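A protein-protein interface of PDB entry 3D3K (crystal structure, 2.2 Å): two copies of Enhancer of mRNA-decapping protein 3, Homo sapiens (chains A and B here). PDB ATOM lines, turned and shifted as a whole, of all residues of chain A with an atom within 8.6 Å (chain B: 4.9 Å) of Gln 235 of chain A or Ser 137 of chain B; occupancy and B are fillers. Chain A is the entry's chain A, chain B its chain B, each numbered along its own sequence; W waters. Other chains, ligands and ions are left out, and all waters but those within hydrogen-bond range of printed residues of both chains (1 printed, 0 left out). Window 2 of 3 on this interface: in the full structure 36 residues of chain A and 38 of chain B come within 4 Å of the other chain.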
ATOM      1  N   LEU A  41       9.853 -10.747  -9.733  1.00  0.00           N
ATOM      2  CA  LEU A  41       9.541  -9.329  -9.876  1.00  0.00           C
ATOM      3  C   LEU A  41       9.155  -8.961 -11.310  1.00  0.00           C
ATOM      4  O   LEU A  41       8.119  -8.338 -11.530  1.00  0.00           O
ATOM      5  CB  LEU A  41      10.735  -8.487  -9.414  1.00  0.00           C
ATOM      6  CG  LEU A  41      10.756  -6.977  -9.662  1.00  0.00           C
ATOM      7  CD1 LEU A  41       9.664  -6.255  -8.850  1.00  0.00           C
ATOM      8  CD2 LEU A  41      12.140  -6.427  -9.336  1.00  0.00           C
ATOM      9  N   VAL A  44       5.786 -10.524 -12.535  1.00  0.00           N
ATOM     10  CA  VAL A  44       4.666  -9.749 -12.023  1.00  0.00           C
ATOM     11  C   VAL A  44       4.529  -8.425 -12.801  1.00  0.00           C
ATOM     12  O   VAL A  44       3.415  -8.024 -13.156  1.00  0.00           O
ATOM     13  CB  VAL A  44       4.803  -9.538 -10.489  1.00  0.00           C
ATOM     14  CG1 VAL A  44       3.745  -8.597  -9.953  1.00  0.00           C
ATOM     15  CG2 VAL A  44       4.722 -10.878  -9.772  1.00  0.00           C
ATOM     16  N   ALA A  45       5.664  -7.777 -13.082  1.00  0.00           N
ATOM     17  CA  ALA A  45       5.695  -6.562 -13.901  1.00  0.00           C
ATOM     18  C   ALA A  45       5.071  -6.803 -15.270  1.00  0.00           C
ATOM     19  O   ALA A  45       4.271  -6.003 -15.735  1.00  0.00           O
ATOM     20  CB  ALA A  45       7.118  -6.038 -14.047  1.00  0.00           C
ATOM     21  N   HIS A  48       1.234  -7.206 -15.317  1.00  0.00           N
ATOM     22  CA  HIS A  48       0.548  -5.929 -15.235  1.00  0.00           C
ATOM     23  C   HIS A  48       0.766  -5.010 -16.451  1.00  0.00           C
ATOM     24  O   HIS A  48       0.298  -3.868 -16.460  1.00  0.00           O
ATOM     25  CB  HIS A  48       0.888  -5.233 -13.912  1.00  0.00           C
ATOM     26  CG  HIS A  48       0.445  -6.000 -12.701  1.00  0.00           C
ATOM     27  ND1 HIS A  48      -0.851  -6.441 -12.527  1.00  0.00           N
ATOM     28  CD2 HIS A  48       1.129  -6.408 -11.605  1.00  0.00           C
ATOM     29  CE1 HIS A  48      -0.948  -7.084 -11.378  1.00  0.00           C
ATOM     30  NE2 HIS A  48       0.239  -7.077 -10.798  1.00  0.00           N
ATOM     31  N   ILE A 232       9.392  -0.187 -13.656  1.00  0.00           N
ATOM     32  CA  ILE A 232       8.597  -0.942 -12.681  1.00  0.00           C
ATOM     33  C   ILE A 232       7.960  -0.014 -11.649  1.00  0.00           C
ATOM     34  O   ILE A 232       8.672   0.699 -10.924  1.00  0.00           O
ATOM     35  CB  ILE A 232       9.428  -2.055 -11.956  1.00  0.00           C
ATOM     36  CG1 ILE A 232      10.097  -2.998 -12.962  1.00  0.00           C
ATOM     37  CG2 ILE A 232       8.539  -2.872 -11.024  1.00  0.00           C
ATOM     38  CD1 ILE A 232      11.215  -3.863 -12.355  1.00  0.00           C
ATOM     39  N   PRO A 233       6.611  -0.001 -11.600  1.00  0.00           N
ATOM     40  CA  PRO A 233       5.853   0.733 -10.601  1.00  0.00           C
ATOM     41  C   PRO A 233       6.051   0.159  -9.193  1.00  0.00           C
ATOM     42  O   PRO A 233       6.343  -1.027  -9.041  1.00  0.00           O
ATOM     43  CB  PRO A 233       4.403   0.534 -11.053  1.00  0.00           C
ATOM     44  CG  PRO A 233       4.494   0.137 -12.480  1.00  0.00           C
ATOM     45  CD  PRO A 233       5.716  -0.689 -12.547  1.00  0.00           C
ATOM     46  N   GLN A 234       5.881   1.017  -8.191  1.00  0.00           N
ATOM     47  CA  GLN A 234       6.110   0.683  -6.790  1.00  0.00           C
ATOM     48  C   GLN A 234       5.351  -0.553  -6.305  1.00  0.00           C
ATOM     49  O   GLN A 234       5.932  -1.404  -5.636  1.00  0.00           O
ATOM     50  CB  GLN A 234       5.764   1.888  -5.911  1.00  0.00           C
ATOM     51  CG  GLN A 234       6.004   1.705  -4.416  1.00  0.00           C
ATOM     52  CD  GLN A 234       5.578   2.920  -3.620  1.00  0.00           C
ATOM     53  OE1 GLN A 234       4.460   3.419  -3.767  1.00  0.00           O
ATOM     54  NE2 GLN A 234       6.470   3.407  -2.767  1.00  0.00           N
ATOM     55  N   GLN A 235       4.068  -0.649  -6.648  1.00  0.00           N
ATOM     56  CA  GLN A 235       3.205  -1.735  -6.162  1.00  0.00           C
ATOM     57  C   GLN A 235       3.551  -3.124  -6.690  1.00  0.00           C
ATOM     58  O   GLN A 235       3.190  -4.121  -6.070  1.00  0.00           O
ATOM     59  CB  GLN A 235       1.729  -1.423  -6.420  1.00  0.00           C
ATOM     60  CG  GLN A 235       1.183  -0.268  -5.582  1.00  0.00           C
ATOM     61  CD  GLN A 235      -0.208   0.150  -6.014  1.00  0.00           C
ATOM     62  OE1 GLN A 235      -1.089  -0.689  -6.229  1.00  0.00           O
ATOM     63  NE2 GLN A 235      -0.413   1.456  -6.153  1.00  0.00           N
ATOM     64  N   VAL A 236       4.247  -3.186  -7.828  1.00  0.00           N
ATOM     65  CA  VAL A 236       4.766  -4.456  -8.373  1.00  0.00           C
ATOM     66  C   VAL A 236       5.836  -5.041  -7.447  1.00  0.00           C
ATOM     67  O   VAL A 236       5.891  -6.257  -7.229  1.00  0.00           O
ATOM     68  CB  VAL A 236       5.344  -4.285  -9.810  1.00  0.00           C
ATOM     69  CG1 VAL A 236       6.102  -5.524 -10.245  1.00  0.00           C
ATOM     70  CG2 VAL A 236       4.237  -3.980 -10.802  1.00  0.00           C
ATOM     71  N   PHE A 237       6.681  -4.165  -6.908  1.00  0.00           N
ATOM     72  CA  PHE A 237       7.674  -4.557  -5.921  1.00  0.00           C
ATOM     73  C   PHE A 237       6.968  -5.089  -4.674  1.00  0.00           C
ATOM     74  O   PHE A 237       7.341  -6.131  -4.143  1.00  0.00           O
ATOM     75  CB  PHE A 237       8.557  -3.374  -5.537  1.00  0.00           C
ATOM     76  CG  PHE A 237       9.532  -2.954  -6.603  1.00  0.00           C
ATOM     77  CD1 PHE A 237      10.768  -3.583  -6.723  1.00  0.00           C
ATOM     78  CD2 PHE A 237       9.235  -1.893  -7.457  1.00  0.00           C
ATOM     79  CE1 PHE A 237      11.682  -3.178  -7.696  1.00  0.00           C
ATOM     80  CE2 PHE A 237      10.141  -1.485  -8.430  1.00  0.00           C
ATOM     81  CZ  PHE A 237      11.364  -2.126  -8.550  1.00  0.00           C
ATOM     82  N   GLN A 238       5.935  -4.368  -4.231  1.00  0.00           N
ATOM     83  CA  GLN A 238       5.174  -4.734  -3.034  1.00  0.00           C
ATOM     84  C   GLN A 238       4.534  -6.121  -3.164  1.00  0.00           C
ATOM     85  O   GLN A 238       4.483  -6.887  -2.194  1.00  0.00           O
ATOM     86  CB  GLN A 238       4.128  -3.653  -2.700  1.00  0.00           C
ATOM     87  CG  GLN A 238       4.748  -2.264  -2.431  1.00  0.00           C
ATOM     88  CD  GLN A 238       3.737  -1.177  -2.067  1.00  0.00           C
ATOM     89  OE1 GLN A 238       2.561  -1.235  -2.444  1.00  0.00           O
ATOM     90  NE2 GLN A 238       4.202  -0.167  -1.328  1.00  0.00           N
ATOM     91  N   GLU A 239       4.078  -6.444  -4.370  1.00  0.00           N
ATOM     92  CA  GLU A 239       3.437  -7.728  -4.664  1.00  0.00           C
ATOM     93  C   GLU A 239       4.383  -8.929  -4.532  1.00  0.00           C
ATOM     94  O   GLU A 239       3.933 -10.067  -4.367  1.00  0.00           O
ATOM     95  CB  GLU A 239       2.816  -7.690  -6.064  1.00  0.00           C
ATOM     96  CG  GLU A 239       1.909  -8.871  -6.379  1.00  0.00           C
ATOM     97  CD  GLU A 239       1.087  -8.671  -7.635  1.00  0.00           C
ATOM     98  OE1 GLU A 239       0.844  -7.495  -8.018  1.00  0.00           O
ATOM     99  OE2 GLU A 239       0.682  -9.698  -8.230  1.00  0.00           O
ATOM    100  N   VAL A 240       5.687  -8.678  -4.625  1.00  0.00           N
ATOM    101  CA  VAL A 240       6.679  -9.739  -4.420  1.00  0.00           C
ATOM    102  C   VAL A 240       7.353  -9.619  -3.045  1.00  0.00           C
ATOM    103  O   VAL A 240       8.343 -10.293  -2.764  1.00  0.00           O
ATOM    104  CB  VAL A 240       7.711  -9.851  -5.597  1.00  0.00           C
ATOM    105  CG1 VAL A 240       6.998 -10.233  -6.893  1.00  0.00           C
ATOM    106  CG2 VAL A 240       8.515  -8.568  -5.782  1.00  0.00           C
ATOM    107  N   GLY A 241       6.788  -8.763  -2.193  1.00  0.00           N
ATOM    108  CA  GLY A 241       7.228  -8.630  -0.809  1.00  0.00           C
ATOM    109  C   GLY A 241       8.433  -7.731  -0.624  1.00  0.00           C
ATOM    110  O   GLY A 241       9.146  -7.843   0.371  1.00  0.00           O
ATOM    111  N   ILE A 242       8.665  -6.846  -1.588  1.00  0.00           N
ATOM    112  CA  ILE A 242       9.715  -5.844  -1.473  1.00  0.00           C
ATOM    113  C   ILE A 242       9.078  -4.506  -1.115  1.00  0.00           C
ATOM    114  O   ILE A 242       8.235  -3.999  -1.859  1.00  0.00           O
ATOM    115  CB  ILE A 242      10.543  -5.708  -2.783  1.00  0.00           C
ATOM    116  CG1 ILE A 242      11.252  -7.027  -3.120  1.00  0.00           C
ATOM    117  CG2 ILE A 242      11.548  -4.552  -2.677  1.00  0.00           C
ATOM    118  CD1 ILE A 242      11.900  -7.048  -4.495  1.00  0.00           C
ATOM    119  N   TYR A 244       9.456  -1.070  -1.410  1.00  0.00           N
ATOM    120  CA  TYR A 244      10.279  -0.306  -2.340  1.00  0.00           C
ATOM    121  C   TYR A 244       9.966   1.182  -2.333  1.00  0.00           C
ATOM    122  O   TYR A 244       8.803   1.596  -2.428  1.00  0.00           O
ATOM    123  CB  TYR A 244      10.125  -0.861  -3.759  1.00  0.00           C
ATOM    124  CG  TYR A 244      10.858  -0.092  -4.848  1.00  0.00           C
ATOM    125  CD1 TYR A 244      12.157  -0.444  -5.224  1.00  0.00           C
ATOM    126  CD2 TYR A 244      10.245   0.973  -5.516  1.00  0.00           C
ATOM    127  CE1 TYR A 244      12.830   0.258  -6.221  1.00  0.00           C
ATOM    128  CE2 TYR A 244      10.910   1.677  -6.515  1.00  0.00           C
ATOM    129  CZ  TYR A 244      12.198   1.313  -6.861  1.00  0.00           C
ATOM    130  OH  TYR A 244      12.853   2.008  -7.854  1.00  0.00           O
ATOM    131  N   LEU B 133      -2.793   2.570 -18.378  1.00  0.00           N
ATOM    132  CA  LEU B 133      -3.512   2.728 -17.109  1.00  0.00           C
ATOM    133  C   LEU B 133      -3.234   1.594 -16.141  1.00  0.00           C
ATOM    134  O   LEU B 133      -3.172   1.814 -14.928  1.00  0.00           O
ATOM    135  CB  LEU B 133      -5.032   2.836 -17.336  1.00  0.00           C
ATOM    136  CG  LEU B 133      -5.591   4.152 -17.877  1.00  0.00           C
ATOM    137  CD1 LEU B 133      -7.095   4.047 -18.067  1.00  0.00           C
ATOM    138  CD2 LEU B 133      -5.255   5.310 -16.941  1.00  0.00           C
ATOM    139  N   SER B 134      -3.100   0.384 -16.681  1.00  0.00           N
ATOM    140  CA  SER B 134      -2.783  -0.805 -15.892  1.00  0.00           C
ATOM    141  C   SER B 134      -1.467  -0.622 -15.144  1.00  0.00           C
ATOM    142  O   SER B 134      -1.361  -0.966 -13.969  1.00  0.00           O
ATOM    143  CB  SER B 134      -2.702  -2.038 -16.800  1.00  0.00           C
ATOM    144  OG  SER B 134      -2.410  -3.207 -16.055  1.00  0.00           O
ATOM    145  N   LEU B 135      -0.467  -0.079 -15.831  1.00  0.00           N
ATOM    146  CA  LEU B 135       0.817   0.229 -15.193  1.00  0.00           C
ATOM    147  C   LEU B 135       0.724   1.421 -14.245  1.00  0.00           C
ATOM    148  O   LEU B 135       1.261   1.379 -13.131  1.00  0.00           O
ATOM    149  CB  LEU B 135       1.911   0.430 -16.247  1.00  0.00           C
ATOM    150  CG  LEU B 135       2.345  -0.866 -16.950  1.00  0.00           C
ATOM    151  CD1 LEU B 135       3.241  -0.581 -18.172  1.00  0.00           C
ATOM    152  CD2 LEU B 135       3.031  -1.813 -15.958  1.00  0.00           C
ATOM    153  N   PHE B 136       0.016   2.463 -14.673  1.00  0.00           N
ATOM    154  CA  PHE B 136      -0.160   3.667 -13.866  1.00  0.00           C
ATOM    155  C   PHE B 136      -0.898   3.379 -12.557  1.00  0.00           C
ATOM    156  O   PHE B 136      -0.628   4.018 -11.536  1.00  0.00           O
ATOM    157  CB  PHE B 136      -0.886   4.753 -14.670  1.00  0.00           C
ATOM    158  CG  PHE B 136      -1.005   6.066 -13.951  1.00  0.00           C
ATOM    159  CD1 PHE B 136      -0.038   7.058 -14.122  1.00  0.00           C
ATOM    160  CD2 PHE B 136      -2.086   6.320 -13.102  1.00  0.00           C
ATOM    161  CE1 PHE B 136      -0.144   8.272 -13.456  1.00  0.00           C
ATOM    162  CE2 PHE B 136      -2.197   7.534 -12.430  1.00  0.00           C
ATOM    163  CZ  PHE B 136      -1.228   8.510 -12.606  1.00  0.00           C
ATOM    164  N   SER B 137      -1.821   2.418 -12.595  1.00  0.00           N
ATOM    165  CA  SER B 137      -2.564   1.969 -11.409  1.00  0.00           C
ATOM    166  C   SER B 137      -1.669   1.387 -10.329  1.00  0.00           C
ATOM    167  O   SER B 137      -2.043   1.366  -9.162  1.00  0.00           O
ATOM    168  CB  SER B 137      -3.623   0.927 -11.792  1.00  0.00           C
ATOM    169  OG  SER B 137      -4.686   1.550 -12.495  1.00  0.00           O
ATOM    170  N   LYS B 138      -0.500   0.895 -10.727  1.00  0.00           N
ATOM    171  CA  LYS B 138       0.433   0.280  -9.790  1.00  0.00           C
ATOM    172  C   LYS B 138       1.458   1.297  -9.282  1.00  0.00           C
ATOM    173  O   LYS B 138       2.365   0.953  -8.525  1.00  0.00           O
ATOM    174  CB  LYS B 138       1.107  -0.946 -10.418  1.00  0.00           C
ATOM    175  CG  LYS B 138       0.137  -2.075 -10.800  1.00  0.00           C
ATOM    176  CD  LYS B 138      -0.317  -2.866  -9.576  1.00  0.00           C
ATOM    177  CE  LYS B 138      -1.568  -3.674  -9.874  1.00  0.00           C
ATOM    178  NZ  LYS B 138      -1.942  -4.549  -8.720  1.00  0.00           N
ATOM    179  N   THR B 139       1.302   2.554  -9.691  1.00  0.00           N
ATOM    180  CA  THR B 139       2.134   3.631  -9.143  1.00  0.00           C
ATOM    181  C   THR B 139       1.409   4.291  -7.971  1.00  0.00           C
ATOM    182  O   THR B 139       0.309   3.878  -7.593  1.00  0.00           O
ATOM    183  CB  THR B 139       2.525   4.698 -10.204  1.00  0.00           C
ATOM    184  OG1 THR B 139       1.399   5.534 -10.510  1.00  0.00           O
ATOM    185  CG2 THR B 139       3.055   4.045 -11.486  1.00  0.00           C
ATOM    186  N   GLN B 140       2.037   5.313  -7.402  1.00  0.00           N
ATOM    187  CA  GLN B 140       1.410   6.151  -6.390  1.00  0.00           C
ATOM    188  C   GLN B 140       0.617   7.296  -7.029  1.00  0.00           C
ATOM    189  O   GLN B 140       0.038   8.133  -6.326  1.00  0.00           O
ATOM    190  CB  GLN B 140       2.452   6.678  -5.392  1.00  0.00           C
ATOM    191  CG  GLN B 140       3.707   7.302  -6.012  1.00  0.00           C
ATOM    192  CD  GLN B 140       4.772   6.282  -6.422  1.00  0.00           C
ATOM    193  OE1 GLN B 140       4.692   5.682  -7.493  1.00  0.00           O
ATOM    194  NE2 GLN B 140       5.792   6.111  -5.577  1.00  0.00           N
ATOM    195  N   GLN B 143      -5.463   8.650 -10.484  1.00  0.00           N
ATOM    196  CA  GLN B 143      -6.291   8.781 -11.685  1.00  0.00           C
ATOM    197  C   GLN B 143      -7.655   9.361 -11.317  1.00  0.00           C
ATOM    198  O   GLN B 143      -8.326   8.853 -10.421  1.00  0.00           O
ATOM    199  CB  GLN B 143      -6.467   7.435 -12.407  1.00  0.00           C
ATOM    200  CG  GLN B 143      -7.310   7.541 -13.684  1.00  0.00           C
ATOM    201  CD  GLN B 143      -7.717   6.212 -14.270  1.00  0.00           C
ATOM    202  OE1 GLN B 143      -7.172   5.164 -13.928  1.00  0.00           O
ATOM    203  NE2 GLN B 143      -8.695   6.247 -15.169  1.00  0.00           N
HETATM  204  O   HOH W   1       5.786   3.847  -8.877  1.00  0.00           O
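No position is printed for both chains. Of the 11 pairs that touch across the chains among the printed residues, none has its exchanged pair printed and touching as well.
O of His 48 of chain A is in hydrogen-bond range of OG of Ser 134 of chain B (2.8 Å). NE2 of Gln 235 of chain A lies within hydrogen-bond range of O of Thr 139 of chain B, at 2.9 Å. O of Ser 137 of chain B sits at hydrogen-bond distance from NE2 of Gln 235 of chain A, at 3.4 Å. N of Gln 235 of chain A is in hydrogen-bond range of O of Lys 138 of chain B, at 3.0 Å.
O of Phe 136 of chain B lies within hydrogen-bond range of OG1 of Thr 139 of chain B, 2.7 Å away. O of Leu 133 of chain B sits at hydrogen-bond distance from OG of Ser 137 of chain B. The side-chain amide nitrogen (NE2) of Gln 234 of chain A is in hydrogen-bond range of the backbone carbonyl oxygen (O) of Tyr 244 of chain A, at 3.0 Å. The side-chain carboxylate of Glu 239 of chain A sits at hydrogen-bond distance from a ring nitrogen (NE2) of His 48 of chain A, at 2.9 Å.
Of the 9 printed residues of chain B, 6 touch a printed residue of chain A. Hydrophobic or aromatic side chains of chain A within 4 Å of the printed part of chain B: His 48 and Pro 233. Among the printed residues, 11 pairs touch across the chains.
Water W1 bridges the side-chain amide oxygen of Gln 140 of chain B and the backbone NH of Gln 234 of chain A.
Of the printed residues of chain B, Pro 233 of chain A touches Leu 135 (3.5 Å), Lys 138 (3.3 Å) and Thr 139 (3.8 Å). Gln 235 of chain A touches three residues of chain B. Of the printed residues of chain A, Ser 134 of chain B touches His 48. Printed residues of chain A within 4 Å of Ser 137 of chain B: Gln 235. Printed residues of chain A within 4 Å of Thr 139 of chain B: Pro 233 and Gln 235. The nearest residue of chain B that does not touch Gln 235 of chain A is Gln 140 of chain B (4.7 Å). The nearest printed residue of chain A that does not touch Thr 139 of chain B is Gln 234 of chain A (4.7 Å).
CD2 of Leu 135 of chain B touches O of His 48 of chain A, 3.5 Å away. CE1 of His 48 of chain A touches CE of Lys 138 of chain B, at 3.8 Å. Leu 135 of chain B touches Pro 233 of chain A (O to CG, 3.5 Å). Pro 233 of chain A touches Lys 138 of chain B (CB to O, 3.3 Å). CB of Pro 233 of chain A touches CG2 of Thr 139 of chain B (3.8 Å). N of Gln 234 of chain A touches O of Lys 138 of chain B, at 3.5 Å. Gln 234 of chain A touches Gln 140 of chain B.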
